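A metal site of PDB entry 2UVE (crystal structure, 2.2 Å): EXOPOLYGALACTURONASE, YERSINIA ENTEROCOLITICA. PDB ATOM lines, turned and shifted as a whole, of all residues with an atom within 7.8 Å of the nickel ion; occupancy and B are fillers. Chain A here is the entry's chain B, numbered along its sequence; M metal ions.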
ATOM      1  N   LYS A 254       9.185  23.387  12.868  1.00  0.00           N
ATOM      2  CA  LYS A 254       9.749  24.609  12.303  1.00  0.00           C
ATOM      3  C   LYS A 254       8.794  25.813  12.340  1.00  0.00           C
ATOM      4  O   LYS A 254       7.591  25.670  12.212  1.00  0.00           O
ATOM      5  CB  LYS A 254      10.326  24.346  10.898  1.00  0.00           C
ATOM      6  CG  LYS A 254       9.350  24.445   9.778  1.00  0.00           C
ATOM      7  CD  LYS A 254       9.845  23.554   8.629  1.00  0.00           C
ATOM      8  CE  LYS A 254       9.169  23.900   7.333  1.00  0.00           C
ATOM      9  NZ  LYS A 254       9.911  25.055   6.721  1.00  0.00           N
ATOM     10  N   PRO A 255       9.349  27.022  12.513  1.00  0.00           N
ATOM     11  CA  PRO A 255       8.532  28.239  12.537  1.00  0.00           C
ATOM     12  C   PRO A 255       7.598  28.392  11.323  1.00  0.00           C
ATOM     13  O   PRO A 255       8.040  28.223  10.159  1.00  0.00           O
ATOM     14  CB  PRO A 255       9.558  29.348  12.623  1.00  0.00           C
ATOM     15  CG  PRO A 255      10.794  28.671  13.207  1.00  0.00           C
ATOM     16  CD  PRO A 255      10.795  27.302  12.673  1.00  0.00           C
ATOM     17  N   GLU A 340       5.012  31.147  13.871  1.00  0.00           N
ATOM     18  CA  GLU A 340       5.341  32.478  13.368  1.00  0.00           C
ATOM     19  C   GLU A 340       4.269  33.443  13.954  1.00  0.00           C
ATOM     20  O   GLU A 340       3.101  33.373  13.544  1.00  0.00           O
ATOM     21  CB  GLU A 340       5.265  32.449  11.829  1.00  0.00           C
ATOM     22  CG  GLU A 340       5.513  33.813  11.132  1.00  0.00           C
ATOM     23  CD  GLU A 340       6.957  34.206  11.190  1.00  0.00           C
ATOM     24  OE1 GLU A 340       7.808  33.342  11.461  1.00  0.00           O
ATOM     25  OE2 GLU A 340       7.272  35.406  11.001  1.00  0.00           O
ATOM     26  N   GLU A 361      11.147  27.117  19.127  1.00  0.00           N
ATOM     27  CA  GLU A 361      11.233  27.353  17.656  1.00  0.00           C
ATOM     28  C   GLU A 361      10.148  28.286  17.194  1.00  0.00           C
ATOM     29  O   GLU A 361       9.430  27.973  16.230  1.00  0.00           O
ATOM     30  CB  GLU A 361      11.202  26.053  16.833  1.00  0.00           C
ATOM     31  CG  GLU A 361      12.405  25.115  17.048  1.00  0.00           C
ATOM     32  CD  GLU A 361      12.499  23.997  15.977  1.00  0.00           C
ATOM     33  OE1 GLU A 361      12.614  24.328  14.743  1.00  0.00           O
ATOM     34  OE2 GLU A 361      12.455  22.774  16.363  1.00  0.00           O
ATOM     35  N   ASN A 362       9.950  29.406  17.903  1.00  0.00           N
ATOM     36  CA  ASN A 362       8.935  30.407  17.494  1.00  0.00           C
ATOM     37  C   ASN A 362       9.612  31.652  16.940  1.00  0.00           C
ATOM     38  O   ASN A 362      10.824  31.866  17.204  1.00  0.00           O
ATOM     39  CB  ASN A 362       8.023  30.799  18.674  1.00  0.00           C
ATOM     40  CG  ASN A 362       7.121  29.642  19.159  1.00  0.00           C
ATOM     41  OD1 ASN A 362       6.856  28.697  18.425  1.00  0.00           O
ATOM     42  ND2 ASN A 362       6.616  29.740  20.373  1.00  0.00           N
ATOM     43  N   HIS A 363       8.868  32.457  16.180  1.00  0.00           N
ATOM     44  CA  HIS A 363       9.351  33.787  15.809  1.00  0.00           C
ATOM     45  C   HIS A 363       8.334  34.816  16.233  1.00  0.00           C
ATOM     46  O   HIS A 363       7.139  34.590  16.102  1.00  0.00           O
ATOM     47  CB  HIS A 363       9.460  33.961  14.276  1.00  0.00           C
ATOM     48  CG  HIS A 363      10.444  33.096  13.584  1.00  0.00           C
ATOM     49  ND1 HIS A 363      10.328  32.814  12.243  1.00  0.00           N
ATOM     50  CD2 HIS A 363      11.596  32.503  14.004  1.00  0.00           C
ATOM     51  CE1 HIS A 363      11.357  32.079  11.854  1.00  0.00           C
ATOM     52  NE2 HIS A 363      12.145  31.888  12.902  1.00  0.00           N
ATOM     53  N   ASN A 387      15.468  28.143  21.126  1.00  0.00           N
ATOM     54  CA  ASN A 387      15.779  28.219  19.678  1.00  0.00           C
ATOM     55  C   ASN A 387      14.781  29.074  18.933  1.00  0.00           C
ATOM     56  O   ASN A 387      14.259  28.692  17.875  1.00  0.00           O
ATOM     57  CB  ASN A 387      15.859  26.801  19.058  1.00  0.00           C
ATOM     58  CG  ASN A 387      16.938  25.940  19.710  1.00  0.00           C
ATOM     59  OD1 ASN A 387      18.111  25.971  19.323  1.00  0.00           O
ATOM     60  ND2 ASN A 387      16.564  25.270  20.759  1.00  0.00           N
ATOM     61  N   SER A 388      14.452  30.224  19.525  1.00  0.00           N
ATOM     62  CA  SER A 388      13.447  31.130  18.974  1.00  0.00           C
ATOM     63  C   SER A 388      14.140  32.407  18.522  1.00  0.00           C
ATOM     64  O   SER A 388      15.267  32.646  18.903  1.00  0.00           O
ATOM     65  CB  SER A 388      12.377  31.433  20.052  1.00  0.00           C
ATOM     66  OG  SER A 388      11.527  30.324  20.227  1.00  0.00           O
ATOM     67  N   GLN A 389      13.444  33.233  17.731  1.00  0.00           N
ATOM     68  CA  GLN A 389      13.991  34.537  17.326  1.00  0.00           C
ATOM     69  C   GLN A 389      13.029  35.622  17.506  1.00  0.00           C
ATOM     70  O   GLN A 389      11.895  35.488  17.123  1.00  0.00           O
ATOM     71  CB  GLN A 389      14.537  34.608  15.880  1.00  0.00           C
ATOM     72  CG  GLN A 389      15.872  33.864  15.676  1.00  0.00           C
ATOM     73  CD  GLN A 389      15.584  32.464  15.225  1.00  0.00           C
ATOM     74  OE1 GLN A 389      14.713  32.287  14.386  1.00  0.00           O
ATOM     75  NE2 GLN A 389      16.297  31.454  15.768  1.00  0.00           N
ATOM     76  N   GLU A 419      18.848  26.309  15.079  1.00  0.00           N
ATOM     77  CA  GLU A 419      18.873  27.761  15.077  1.00  0.00           C
ATOM     78  C   GLU A 419      19.198  28.316  16.468  1.00  0.00           C
ATOM     79  O   GLU A 419      18.782  27.739  17.478  1.00  0.00           O
ATOM     80  CB  GLU A 419      17.549  28.302  14.580  1.00  0.00           C
ATOM     81  CG  GLU A 419      17.255  28.012  13.100  1.00  0.00           C
ATOM     82  CD  GLU A 419      15.890  28.540  12.724  1.00  0.00           C
ATOM     83  OE1 GLU A 419      15.242  28.038  11.763  1.00  0.00           O
ATOM     84  OE2 GLU A 419      15.464  29.472  13.449  1.00  0.00           O
ATOM     85  N   PRO A 420      19.923  29.438  16.496  1.00  0.00           N
ATOM     86  CA  PRO A 420      20.268  30.094  17.753  1.00  0.00           C
ATOM     87  C   PRO A 420      18.994  30.688  18.371  1.00  0.00           C
ATOM     88  O   PRO A 420      17.984  30.987  17.672  1.00  0.00           O
ATOM     89  CB  PRO A 420      21.227  31.240  17.307  1.00  0.00           C
ATOM     90  CG  PRO A 420      20.851  31.517  15.880  1.00  0.00           C
ATOM     91  CD  PRO A 420      20.395  30.208  15.313  1.00  0.00           C
HETATM   92 NI    NI M   1      13.938  30.660  13.029  1.00  0.00          NI
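The backbone carbonyl oxygen (O) of Glu 419 lies close to the side-chain amide oxygen (OD1) of Asn 387 (2.6 Å). OE1 of Glu 340 is in hydrogen-bond range of ND1 of His 363. The backbone carbonyl oxygen of Asn 362 lies within hydrogen-bond range of the backbone NH of Gln 389, at 3.0 Å. The backbone carbonyl oxygen of Pro 420 lies within hydrogen-bond range of the side-chain amide nitrogen of Gln 389.
The nickel ion is bound by the side-chain carboxylate (OE2) of Glu 419 (2.0 Å), a ring nitrogen (NE2) of His 363 (2.2 Å) and the side-chain amide oxygen (OE1) of Gln 389 (2.3 Å). The nickel ion has three donor atoms within binding distance.
Merely in contact with the nickel ion: Pro 255. Of the 11 residues printed, 4 come within 4 Å of the nickel ion.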
